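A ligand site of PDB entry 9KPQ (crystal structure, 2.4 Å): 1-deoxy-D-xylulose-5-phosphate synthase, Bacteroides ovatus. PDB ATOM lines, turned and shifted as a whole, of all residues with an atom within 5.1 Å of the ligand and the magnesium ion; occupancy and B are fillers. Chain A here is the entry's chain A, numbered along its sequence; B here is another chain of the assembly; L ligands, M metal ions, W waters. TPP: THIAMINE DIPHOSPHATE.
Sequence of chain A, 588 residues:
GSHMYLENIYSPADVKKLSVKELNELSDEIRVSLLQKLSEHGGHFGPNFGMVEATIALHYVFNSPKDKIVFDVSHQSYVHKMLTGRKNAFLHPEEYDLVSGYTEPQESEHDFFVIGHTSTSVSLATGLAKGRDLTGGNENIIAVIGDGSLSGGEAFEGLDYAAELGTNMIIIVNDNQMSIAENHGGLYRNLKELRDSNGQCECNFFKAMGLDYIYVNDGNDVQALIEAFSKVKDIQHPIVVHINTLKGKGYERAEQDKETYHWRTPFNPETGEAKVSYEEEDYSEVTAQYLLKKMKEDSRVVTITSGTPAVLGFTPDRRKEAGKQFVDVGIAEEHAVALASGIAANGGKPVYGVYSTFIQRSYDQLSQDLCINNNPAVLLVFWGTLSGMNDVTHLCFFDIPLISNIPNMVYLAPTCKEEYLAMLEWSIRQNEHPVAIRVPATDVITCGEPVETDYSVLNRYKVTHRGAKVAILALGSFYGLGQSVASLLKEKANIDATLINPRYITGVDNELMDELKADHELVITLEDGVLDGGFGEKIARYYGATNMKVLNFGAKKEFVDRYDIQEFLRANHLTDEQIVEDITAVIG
A nitrogen (N1') of the ligand sits close to the side-chain hydroxyl (OG1) of Thr 118 (3.3 Å). An oxygen (O1A) of the ligand lies close to the backbone NH (N) of Asp 147, 3.5 Å away. N of Thr 118 sits at hydrogen-bond distance from N3' of the ligand, 3.1 Å away. The side-chain amino group of Lys 247 is in salt-bridge range of an oxygen (O1B) of the ligand (2.4 Å). OE2 of Glu 333 is in hydrogen-bond range of N1' of the ligand. N of Gly 148 lies close to O1A of the ligand. The side-chain hydroxyl of Ser 149 sits at hydrogen-bond distance from an oxygen (O2A) of the ligand, at 3.4 Å. A ring nitrogen (ND1) of His 262 is in hydrogen-bond range of an oxygen (O1B) of the ligand (3.0 Å). The backbone carbonyl oxygen of Gly 116 is in hydrogen-bond range of a nitrogen (N4') of the ligand, 3.1 Å away.
OD1 of Asn 183 is in hydrogen-bond range of N of Ser 179, 3.2 Å away. The side-chain carboxylate (OD2) of Asp 147 is in hydrogen-bond range of the backbone NH (N) of Gln 177, 3.4 Å away. A ring nitrogen (ND1) of His 117 is in hydrogen-bond range of the side-chain carboxylate (OD2) of Asp 364 of chain B, 2.9 Å away. The backbone NH of Asp 147 sits at hydrogen-bond distance from the backbone carbonyl oxygen of Asn 174, 3.4 Å away. The guanidinium group (NE) of Arg 361 is in salt-bridge range of the side-chain carboxylate (OD2) of Asp 364 of chain B (2.4 Å). The backbone carbonyl oxygen (O) of Ser 179 lies within hydrogen-bond range of the side-chain amino group (NZ) of Lys 247, 3.0 Å away. N of Met 178 sits close to ND2 of Asn 183 (3.2 Å). The side-chain amino group (NZ) of Lys 247 sits at hydrogen-bond distance from a ring nitrogen (ND1) of His 262.
O1B of the ligand sits close to O of Ser 179 (3.2 Å). Residues that only touch the ligand: Phe 358 (3.1 Å), Gly 146 (3.2 Å), Ile 331 (3.4 Å), His 117 (3.4 Å), Ile 180 (3.7 Å), Pro 47 (3.7 Å), His 75 (3.7 Å), Arg 361 (3.8 Å), Thr 308 (3.9 Å) and His 394 (3.97 Å). Hydrophobic or aromatic side chains within 4 Å of the ligand: Pro 47, His 117, Ile 180, His 262, Ile 331 and Phe 358. 21 residues have an atom within 4 Å of the ligand: Pro 47, His 75, Gly 116, His 117, Thr 118, Gly 146, Asp 147, Gly 148, Ser 149, Asn 176, Met 178, Ser 179, Ile 180, Lys 247, His 262, Thr 308, Ile 331, Glu 333, Phe 358, Arg 361 and His 394. The nearest printed residue that does not touch the ligand is Gly 307 (4.1 Å).
Gly 148 touches the magnesium ion (N to MG, 3.9 Å). Of the 29 residues printed, 4 come within 4 Å of the magnesium ion. The nearest printed residue that does not touch the magnesium ion is Asn 174 (4.1 Å).
The magnesium ion is bound by the side-chain carboxylate of Asp 147 (1.9 Å), an oxygen (O1A) of the ligand (2.0 Å), water W2 (2.1 Å), an oxygen (O3B) of the ligand (2.2 Å), the backbone carbonyl oxygen of Met 178 (2.3 Å) and the side-chain amide oxygen of Asn 176 (2.4 Å).
Water W2 lies within hydrogen-bond range of the backbone carbonyl oxygen of Asn 174 (2.7 Å), the side-chain amide nitrogen of Asn 176 (3.2 Å) and an oxygen (O3A) of the ligand (3.3 Å). Water W1 lies within hydrogen-bond range of O2A of the ligand (2.9 Å), N of Gly 146 (3.0 Å) and OG of Ser 149 (3.3 Å).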
ATOM      1  N   HIS A  44      -2.652  26.068  36.548  1.00  0.00           N
ATOM      2  CA  HIS A  44      -3.582  26.541  35.537  1.00  0.00           C
ATOM      3  C   HIS A  44      -4.240  27.871  35.957  1.00  0.00           C
ATOM      4  O   HIS A  44      -5.255  27.880  36.651  1.00  0.00           O
ATOM      5  CB  HIS A  44      -4.637  25.455  35.240  1.00  0.00           C
ATOM      6  CG  HIS A  44      -4.091  24.285  34.474  1.00  0.00           C
ATOM      7  ND1 HIS A  44      -3.576  23.162  35.083  1.00  0.00           N
ATOM      8  CD2 HIS A  44      -3.930  24.088  33.139  1.00  0.00           C
ATOM      9  CE1 HIS A  44      -3.150  22.318  34.170  1.00  0.00           C
ATOM     10  NE2 HIS A  44      -3.360  22.854  32.975  1.00  0.00           N
ATOM     11  N   PRO A  47      -7.779  29.119  33.487  1.00  0.00           N
ATOM     12  CA  PRO A  47      -9.003  28.325  33.665  1.00  0.00           C
ATOM     13  C   PRO A  47      -9.659  28.489  35.047  1.00  0.00           C
ATOM     14  O   PRO A  47     -10.881  28.434  35.126  1.00  0.00           O
ATOM     15  CB  PRO A  47      -8.513  26.880  33.484  1.00  0.00           C
ATOM     16  CG  PRO A  47      -7.275  26.998  32.643  1.00  0.00           C
ATOM     17  CD  PRO A  47      -6.632  28.281  33.097  1.00  0.00           C
ATOM     18  N   VAL A  73     -11.373  17.334  32.181  1.00  0.00           N
ATOM     19  CA  VAL A  73      -9.920  17.540  32.408  1.00  0.00           C
ATOM     20  C   VAL A  73      -9.535  17.648  33.872  1.00  0.00           C
ATOM     21  O   VAL A  73      -8.690  16.945  34.341  1.00  0.00           O
ATOM     22  CB  VAL A  73      -9.256  18.701  31.615  1.00  0.00           C
ATOM     23  CG1 VAL A  73      -7.780  18.700  31.827  1.00  0.00           C
ATOM     24  CG2 VAL A  73      -9.571  18.636  30.155  1.00  0.00           C
ATOM     25  N   HIS A  75      -8.338  20.342  35.330  1.00  0.00           N
ATOM     26  CA  HIS A  75      -7.366  21.348  35.472  1.00  0.00           C
ATOM     27  C   HIS A  75      -8.066  22.653  35.994  1.00  0.00           C
ATOM     28  O   HIS A  75      -7.369  23.484  36.491  1.00  0.00           O
ATOM     29  CB  HIS A  75      -6.749  21.598  34.083  1.00  0.00           C
ATOM     30  CG  HIS A  75      -7.662  22.342  33.137  1.00  0.00           C
ATOM     31  ND1 HIS A  75      -8.938  21.930  32.838  1.00  0.00           N
ATOM     32  CD2 HIS A  75      -7.484  23.475  32.455  1.00  0.00           C
ATOM     33  CE1 HIS A  75      -9.487  22.768  31.993  1.00  0.00           C
ATOM     34  NE2 HIS A  75      -8.631  23.726  31.758  1.00  0.00           N
ATOM     35  N   GLY A 116      -7.535  13.782  33.756  1.00  0.00           N
ATOM     36  CA  GLY A 116      -6.526  14.678  33.164  1.00  0.00           C
ATOM     37  C   GLY A 116      -6.641  14.817  31.644  1.00  0.00           C
ATOM     38  O   GLY A 116      -6.119  15.787  31.161  1.00  0.00           O
ATOM     39  N   HIS A 117      -7.297  13.852  31.037  1.00  0.00           N
ATOM     40  CA  HIS A 117      -7.425  13.885  29.558  1.00  0.00           C
ATOM     41  C   HIS A 117      -8.714  14.632  29.200  1.00  0.00           C
ATOM     42  O   HIS A 117      -9.538  14.874  30.073  1.00  0.00           O
ATOM     43  CB  HIS A 117      -7.247  12.499  28.941  1.00  0.00           C
ATOM     44  CG  HIS A 117      -5.852  12.007  28.890  1.00  0.00           C
ATOM     45  ND1 HIS A 117      -5.506  10.911  28.149  1.00  0.00           N
ATOM     46  CD2 HIS A 117      -4.729  12.424  29.472  1.00  0.00           C
ATOM     47  CE1 HIS A 117      -4.216  10.683  28.281  1.00  0.00           C
ATOM     48  NE2 HIS A 117      -3.729  11.595  29.076  1.00  0.00           N
ATOM     49  N   THR A 118      -8.881  14.958  27.929  1.00  0.00           N
ATOM     50  CA  THR A 118      -9.991  15.803  27.519  1.00  0.00           C
ATOM     51  C   THR A 118     -11.228  15.036  27.062  1.00  0.00           C
ATOM     52  O   THR A 118     -11.133  13.879  26.617  1.00  0.00           O
ATOM     53  CB  THR A 118      -9.572  16.692  26.376  1.00  0.00           C
ATOM     54  OG1 THR A 118      -9.048  15.865  25.323  1.00  0.00           O
ATOM     55  CG2 THR A 118      -8.516  17.661  26.828  1.00  0.00           C
ATOM     56  N   GLY A 146     -15.385  22.264  29.107  1.00  0.00           N
ATOM     57  CA  GLY A 146     -14.883  23.391  28.320  1.00  0.00           C
ATOM     58  C   GLY A 146     -15.226  23.323  26.836  1.00  0.00           C
ATOM     59  O   GLY A 146     -15.373  22.234  26.283  1.00  0.00           O
ATOM     60  N   ASP A 147     -15.332  24.495  26.208  1.00  0.00           N
ATOM     61  CA  ASP A 147     -15.683  24.628  24.795  1.00  0.00           C
ATOM     62  C   ASP A 147     -14.668  23.957  23.867  1.00  0.00           C
ATOM     63  O   ASP A 147     -15.024  23.421  22.829  1.00  0.00           O
ATOM     64  CB  ASP A 147     -15.831  26.124  24.408  1.00  0.00           C
ATOM     65  CG  ASP A 147     -14.599  26.970  24.762  1.00  0.00           C
ATOM     66  OD1 ASP A 147     -14.139  26.962  25.927  1.00  0.00           O
ATOM     67  OD2 ASP A 147     -14.083  27.667  23.859  1.00  0.00           O
ATOM     68  N   GLY A 148     -13.388  23.988  24.249  1.00  0.00           N
ATOM     69  CA  GLY A 148     -12.401  23.256  23.482  1.00  0.00           C
ATOM     70  C   GLY A 148     -12.575  21.737  23.509  1.00  0.00           C
ATOM     71  O   GLY A 148     -12.433  21.061  22.489  1.00  0.00           O
ATOM     72  N   SER A 149     -12.877  21.214  24.701  1.00  0.00           N
ATOM     73  CA  SER A 149     -13.052  19.765  24.901  1.00  0.00           C
ATOM     74  C   SER A 149     -14.226  19.227  24.071  1.00  0.00           C
ATOM     75  O   SER A 149     -14.337  18.010  23.816  1.00  0.00           O
ATOM     76  CB  SER A 149     -13.292  19.436  26.385  1.00  0.00           C
ATOM     77  OG  SER A 149     -12.075  19.389  27.116  1.00  0.00           O
ATOM     78  N   ASN A 174     -18.701  25.441  29.573  1.00  0.00           N
ATOM     79  CA  ASN A 174     -17.954  26.626  30.007  1.00  0.00           C
ATOM     80  C   ASN A 174     -17.310  27.286  28.788  1.00  0.00           C
ATOM     81  O   ASN A 174     -16.164  26.977  28.419  1.00  0.00           O
ATOM     82  CB  ASN A 174     -16.898  26.242  31.053  1.00  0.00           C
ATOM     83  CG  ASN A 174     -16.073  27.417  31.480  1.00  0.00           C
ATOM     84  OD1 ASN A 174     -16.439  28.559  31.216  1.00  0.00           O
ATOM     85  ND2 ASN A 174     -14.957  27.159  32.144  1.00  0.00           N
ATOM     86  N   ASN A 176     -15.484  29.971  27.081  1.00  0.00           N
ATOM     87  CA  ASN A 176     -14.635  31.164  27.197  1.00  0.00           C
ATOM     88  C   ASN A 176     -13.901  31.502  25.893  1.00  0.00           C
ATOM     89  O   ASN A 176     -12.899  32.220  25.907  1.00  0.00           O
ATOM     90  CB  ASN A 176     -13.611  31.019  28.349  1.00  0.00           C
ATOM     91  CG  ASN A 176     -12.778  29.732  28.256  1.00  0.00           C
ATOM     92  OD1 ASN A 176     -12.561  29.163  27.177  1.00  0.00           O
ATOM     93  ND2 ASN A 176     -12.276  29.282  29.417  1.00  0.00           N
ATOM     94  N   GLN A 177     -14.396  30.956  24.775  1.00  0.00           N
ATOM     95  CA  GLN A 177     -13.849  31.214  23.426  1.00  0.00           C
ATOM     96  C   GLN A 177     -12.349  30.925  23.285  1.00  0.00           C
ATOM     97  O   GLN A 177     -11.653  31.584  22.528  1.00  0.00           O
ATOM     98  CB  GLN A 177     -14.124  32.666  23.016  1.00  0.00           C
ATOM     99  CG  GLN A 177     -15.612  33.049  23.054  1.00  0.00           C
ATOM    100  CD  GLN A 177     -16.051  33.571  24.425  1.00  0.00           C
ATOM    101  OE1 GLN A 177     -15.531  34.580  24.916  1.00  0.00           O
ATOM    102  NE2 GLN A 177     -17.005  32.888  25.042  1.00  0.00           N
ATOM    103  N   MET A 178     -11.869  29.910  23.981  1.00  0.00           N
ATOM    104  CA  MET A 178     -10.436  29.578  23.993  1.00  0.00           C
ATOM    105  C   MET A 178     -10.298  28.103  24.305  1.00  0.00           C
ATOM    106  O   MET A 178     -11.026  27.566  25.129  1.00  0.00           O
ATOM    107  CB  MET A 178      -9.705  30.379  25.062  1.00  0.00           C
ATOM    108  CG  MET A 178      -9.077  31.710  24.668  1.00  0.00           C
ATOM    109  SD  MET A 178      -8.398  31.781  23.013  1.00  0.00           S
ATOM    110  CE  MET A 178      -6.639  31.593  23.307  1.00  0.00           C
ATOM    111  N   SER A 179      -9.371  27.427  23.633  1.00  0.00           N
ATOM    112  CA  SER A 179      -8.950  26.117  24.106  1.00  0.00           C
ATOM    113  C   SER A 179      -7.704  26.385  24.935  1.00  0.00           C
ATOM    114  O   SER A 179      -7.783  27.118  25.922  1.00  0.00           O
ATOM    115  CB  SER A 179      -8.680  25.148  22.943  1.00  0.00           C
ATOM    116  OG  SER A 179      -8.403  23.848  23.396  1.00  0.00           O
ATOM    117  N   ILE A 180      -6.565  25.835  24.531  1.00  0.00           N
ATOM    118  CA  ILE A 180      -5.284  26.387  24.970  1.00  0.00           C
ATOM    119  C   ILE A 180      -4.847  27.577  24.083  1.00  0.00           C
ATOM    120  O   ILE A 180      -4.755  28.724  24.546  1.00  0.00           O
ATOM    121  CB  ILE A 180      -4.149  25.350  24.914  1.00  0.00           C
ATOM    122  CG1 ILE A 180      -4.426  24.172  25.851  1.00  0.00           C
ATOM    123  CG2 ILE A 180      -2.809  26.022  25.201  1.00  0.00           C
ATOM    124  CD1 ILE A 180      -3.255  23.199  25.970  1.00  0.00           C
ATOM    125  N   ASN A 183      -9.728  28.101  19.426  1.00  0.00           N
ATOM    126  CA  ASN A 183     -10.482  26.937  18.985  1.00  0.00           C
ATOM    127  C   ASN A 183     -10.472  26.771  17.453  1.00  0.00           C
ATOM    128  O   ASN A 183     -10.178  27.715  16.719  1.00  0.00           O
ATOM    129  CB  ASN A 183     -11.923  27.045  19.498  1.00  0.00           C
ATOM    130  CG  ASN A 183     -12.002  26.981  21.007  1.00  0.00           C
ATOM    131  OD1 ASN A 183     -11.460  26.073  21.625  1.00  0.00           O
ATOM    132  ND2 ASN A 183     -12.688  27.944  21.613  1.00  0.00           N
ATOM    133  N   LYS A 247     -11.946  34.121  30.324  1.00  0.00           N
ATOM    134  CA  LYS A 247     -10.782  33.360  30.747  1.00  0.00           C
ATOM    135  C   LYS A 247      -9.771  34.231  31.485  1.00  0.00           C
ATOM    136  O   LYS A 247      -9.222  35.185  30.912  1.00  0.00           O
ATOM    137  CB  LYS A 247     -10.114  32.683  29.550  1.00  0.00           C
ATOM    138  CG  LYS A 247      -8.976  31.745  29.925  1.00  0.00           C
ATOM    139  CD  LYS A 247      -9.032  30.473  29.076  1.00  0.00           C
ATOM    140  CE  LYS A 247      -8.139  29.395  29.656  1.00  0.00           C
ATOM    141  NZ  LYS A 247      -7.674  28.432  28.648  1.00  0.00           N
ATOM    142  N   HIS A 262      -2.899  30.154  30.242  1.00  0.00           N
ATOM    143  CA  HIS A 262      -3.562  28.885  30.447  1.00  0.00           C
ATOM    144  C   HIS A 262      -2.815  28.050  31.494  1.00  0.00           C
ATOM    145  O   HIS A 262      -3.432  27.416  32.352  1.00  0.00           O
ATOM    146  CB  HIS A 262      -3.684  28.110  29.118  1.00  0.00           C
ATOM    147  CG  HIS A 262      -4.221  26.719  29.284  1.00  0.00           C
ATOM    148  ND1 HIS A 262      -5.572  26.447  29.250  1.00  0.00           N
ATOM    149  CD2 HIS A 262      -3.596  25.544  29.509  1.00  0.00           C
ATOM    150  CE1 HIS A 262      -5.747  25.149  29.426  1.00  0.00           C
ATOM    151  NE2 HIS A 262      -4.574  24.582  29.588  1.00  0.00           N
ATOM    152  N   SER A 306      -3.053  18.581  17.477  1.00  0.00           N
ATOM    153  CA  SER A 306      -4.386  18.302  17.998  1.00  0.00           C
ATOM    154  C   SER A 306      -4.327  19.201  19.244  1.00  0.00           C
ATOM    155  O   SER A 306      -3.929  18.751  20.344  1.00  0.00           O
ATOM    156  CB  SER A 306      -4.582  16.787  18.280  1.00  0.00           C
ATOM    157  OG  SER A 306      -3.383  16.152  18.738  1.00  0.00           O
ATOM    158  N   GLY A 307      -4.689  20.475  19.067  1.00  0.00           N
ATOM    159  CA  GLY A 307      -4.963  21.412  20.143  1.00  0.00           C
ATOM    160  C   GLY A 307      -3.782  21.756  21.060  1.00  0.00           C
ATOM    161  O   GLY A 307      -3.963  22.408  22.079  1.00  0.00           O
ATOM    162  N   THR A 308      -2.589  21.287  20.727  1.00  0.00           N
ATOM    163  CA  THR A 308      -1.415  21.540  21.562  1.00  0.00           C
ATOM    164  C   THR A 308      -0.236  21.923  20.607  1.00  0.00           C
ATOM    165  O   THR A 308       0.704  21.143  20.445  1.00  0.00           O
ATOM    166  CB  THR A 308      -1.031  20.252  22.400  1.00  0.00           C
ATOM    167  OG1 THR A 308      -0.498  19.224  21.538  1.00  0.00           O
ATOM    168  CG2 THR A 308      -2.249  19.679  23.123  1.00  0.00           C
ATOM    169  N   ILE A 331      -9.045  19.224  19.661  1.00  0.00           N
ATOM    170  CA  ILE A 331      -8.505  18.179  20.512  1.00  0.00           C
ATOM    171  C   ILE A 331      -9.002  16.823  20.025  1.00  0.00           C
ATOM    172  O   ILE A 331      -9.735  16.104  20.718  1.00  0.00           O
ATOM    173  CB  ILE A 331      -8.863  18.439  21.968  1.00  0.00           C
ATOM    174  CG1 ILE A 331      -8.731  19.928  22.275  1.00  0.00           C
ATOM    175  CG2 ILE A 331      -7.930  17.679  22.858  1.00  0.00           C
ATOM    176  CD1 ILE A 331      -9.478  20.351  23.532  1.00  0.00           C
ATOM    177  N   GLU A 333      -7.250  13.786  18.467  1.00  0.00           N
ATOM    178  CA  GLU A 333      -6.123  12.913  18.156  1.00  0.00           C
ATOM    179  C   GLU A 333      -6.449  11.813  17.138  1.00  0.00           C
ATOM    180  O   GLU A 333      -5.626  11.447  16.298  1.00  0.00           O
ATOM    181  CB  GLU A 333      -5.603  12.257  19.428  1.00  0.00           C
ATOM    182  CG  GLU A 333      -4.883  13.199  20.379  1.00  0.00           C
ATOM    183  CD  GLU A 333      -5.816  13.940  21.319  1.00  0.00           C
ATOM    184  OE1 GLU A 333      -7.057  13.888  21.095  1.00  0.00           O
ATOM    185  OE2 GLU A 333      -5.317  14.578  22.280  1.00  0.00           O
ATOM    186  N   PHE A 358      -1.074  11.600  25.182  1.00  0.00           N
ATOM    187  CA  PHE A 358      -2.311  11.895  24.434  1.00  0.00           C
ATOM    188  C   PHE A 358      -2.496  11.003  23.211  1.00  0.00           C
ATOM    189  O   PHE A 358      -3.636  10.686  22.839  1.00  0.00           O
ATOM    190  CB  PHE A 358      -2.360  13.374  24.037  1.00  0.00           C
ATOM    191  CG  PHE A 358      -2.419  14.314  25.208  1.00  0.00           C
ATOM    192  CD1 PHE A 358      -2.942  13.888  26.421  1.00  0.00           C
ATOM    193  CD2 PHE A 358      -1.914  15.600  25.121  1.00  0.00           C
ATOM    194  CE1 PHE A 358      -2.991  14.740  27.516  1.00  0.00           C
ATOM    195  CE2 PHE A 358      -1.957  16.470  26.205  1.00  0.00           C
ATOM    196  CZ  PHE A 358      -2.483  16.040  27.410  1.00  0.00           C
ATOM    197  N   ARG A 361      -5.003   7.883  22.552  1.00  0.00           N
ATOM    198  CA  ARG A 361      -6.379   7.894  22.043  1.00  0.00           C
ATOM    199  C   ARG A 361      -6.517   7.236  20.666  1.00  0.00           C
ATOM    200  O   ARG A 361      -7.623   6.826  20.291  1.00  0.00           O
ATOM    201  CB  ARG A 361      -6.921   9.339  21.932  1.00  0.00           C
ATOM    202  CG  ARG A 361      -7.289  10.035  23.237  1.00  0.00           C
ATOM    203  CD  ARG A 361      -8.604   9.536  23.785  1.00  0.00           C
ATOM    204  NE  ARG A 361      -8.828   9.975  25.165  1.00  0.00           N
ATOM    205  CZ  ARG A 361      -9.414  11.122  25.498  1.00  0.00           C
ATOM    206  NH1 ARG A 361      -9.901  11.952  24.581  1.00  0.00           N
ATOM    207  NH2 ARG A 361      -9.527  11.441  26.775  1.00  0.00           N
ATOM    208  N   HIS A 394      -1.109  12.086  33.209  1.00  0.00           N
ATOM    209  CA  HIS A 394      -0.225  12.528  32.144  1.00  0.00           C
ATOM    210  C   HIS A 394       1.083  11.741  32.047  1.00  0.00           C
ATOM    211  O   HIS A 394       2.069  12.243  31.527  1.00  0.00           O
ATOM    212  CB  HIS A 394       0.078  14.018  32.286  1.00  0.00           C
ATOM    213  CG  HIS A 394      -1.115  14.882  32.063  1.00  0.00           C
ATOM    214  ND1 HIS A 394      -2.092  15.070  33.017  1.00  0.00           N
ATOM    215  CD2 HIS A 394      -1.534  15.569  30.974  1.00  0.00           C
ATOM    216  CE1 HIS A 394      -3.034  15.859  32.538  1.00  0.00           C
ATOM    217  NE2 HIS A 394      -2.727  16.165  31.295  1.00  0.00           N
ATOM    218  N   ASP B 364      -7.243   4.480  25.367  1.00  0.00           N
ATOM    219  CA  ASP B 364      -7.125   5.553  26.357  1.00  0.00           C
ATOM    220  C   ASP B 364      -8.292   5.516  27.356  1.00  0.00           C
ATOM    221  O   ASP B 364      -8.163   5.917  28.524  1.00  0.00           O
ATOM    222  CB  ASP B 364      -7.065   6.939  25.674  1.00  0.00           C
ATOM    223  CG  ASP B 364      -6.563   8.031  26.610  1.00  0.00           C
ATOM    224  OD1 ASP B 364      -5.506   7.848  27.223  1.00  0.00           O
ATOM    225  OD2 ASP B 364      -7.225   9.082  26.736  1.00  0.00           O
HETATM  226  N1' TPP L   1      -5.804  15.809  24.651  1.00  0.00           N
HETATM  227  C2' TPP L   1      -6.133  15.120  25.768  1.00  0.00           C
HETATM  228  CM2 TPP L   1      -6.702  13.758  25.601  1.00  0.00           C
HETATM  229  N3' TPP L   1      -5.969  15.572  27.027  1.00  0.00           N
HETATM  230  C4' TPP L   1      -5.469  16.781  27.204  1.00  0.00           C
HETATM  231  N4' TPP L   1      -5.317  17.208  28.479  1.00  0.00           N
HETATM  232  C5' TPP L   1      -5.099  17.625  26.085  1.00  0.00           C
HETATM  233  C6' TPP L   1      -5.293  17.032  24.842  1.00  0.00           C
HETATM  234  C7' TPP L   1      -4.474  18.993  26.210  1.00  0.00           C
HETATM  235  N3  TPP L   1      -5.199  19.947  27.093  1.00  0.00           N
HETATM  236  C2  TPP L   1      -5.016  20.014  28.409  1.00  0.00           C
HETATM  237  S1  TPP L   1      -5.930  21.235  29.124  1.00  0.00           S
HETATM  238  C5  TPP L   1      -6.568  21.717  27.591  1.00  0.00           C
HETATM  239  C4  TPP L   1      -6.053  20.919  26.585  1.00  0.00           C
HETATM  240  CM4 TPP L   1      -6.321  20.998  25.115  1.00  0.00           C
HETATM  241  C6  TPP L   1      -7.533  22.869  27.477  1.00  0.00           C
HETATM  242  C7  TPP L   1      -8.955  22.438  27.160  1.00  0.00           C
HETATM  243  O7  TPP L   1      -9.683  23.595  26.678  1.00  0.00           O
HETATM  244  PA  TPP L   1     -11.100  24.048  27.232  1.00  0.00           P
HETATM  245  O1A TPP L   1     -11.868  24.908  26.294  1.00  0.00           O
HETATM  246  O2A TPP L   1     -11.799  22.754  27.675  1.00  0.00           O
HETATM  247  O3A TPP L   1     -10.680  24.892  28.555  1.00  0.00           O
HETATM  248  PB  TPP L   1     -10.016  26.285  28.942  1.00  0.00           P
HETATM  249  O1B TPP L   1      -8.532  26.187  28.935  1.00  0.00           O
HETATM  250  O2B TPP L   1     -10.571  26.648  30.397  1.00  0.00           O
HETATM  251  O3B TPP L   1     -10.602  27.269  27.904  1.00  0.00           O
HETATM  252 MG    MG M   1     -12.429  26.815  26.785  1.00  0.00          MG
HETATM  253  O   HOH W   1     -12.698  21.130  29.876  1.00  0.00           O
HETATM  254  O   HOH W   2     -13.518  26.501  28.582  1.00  0.00           O
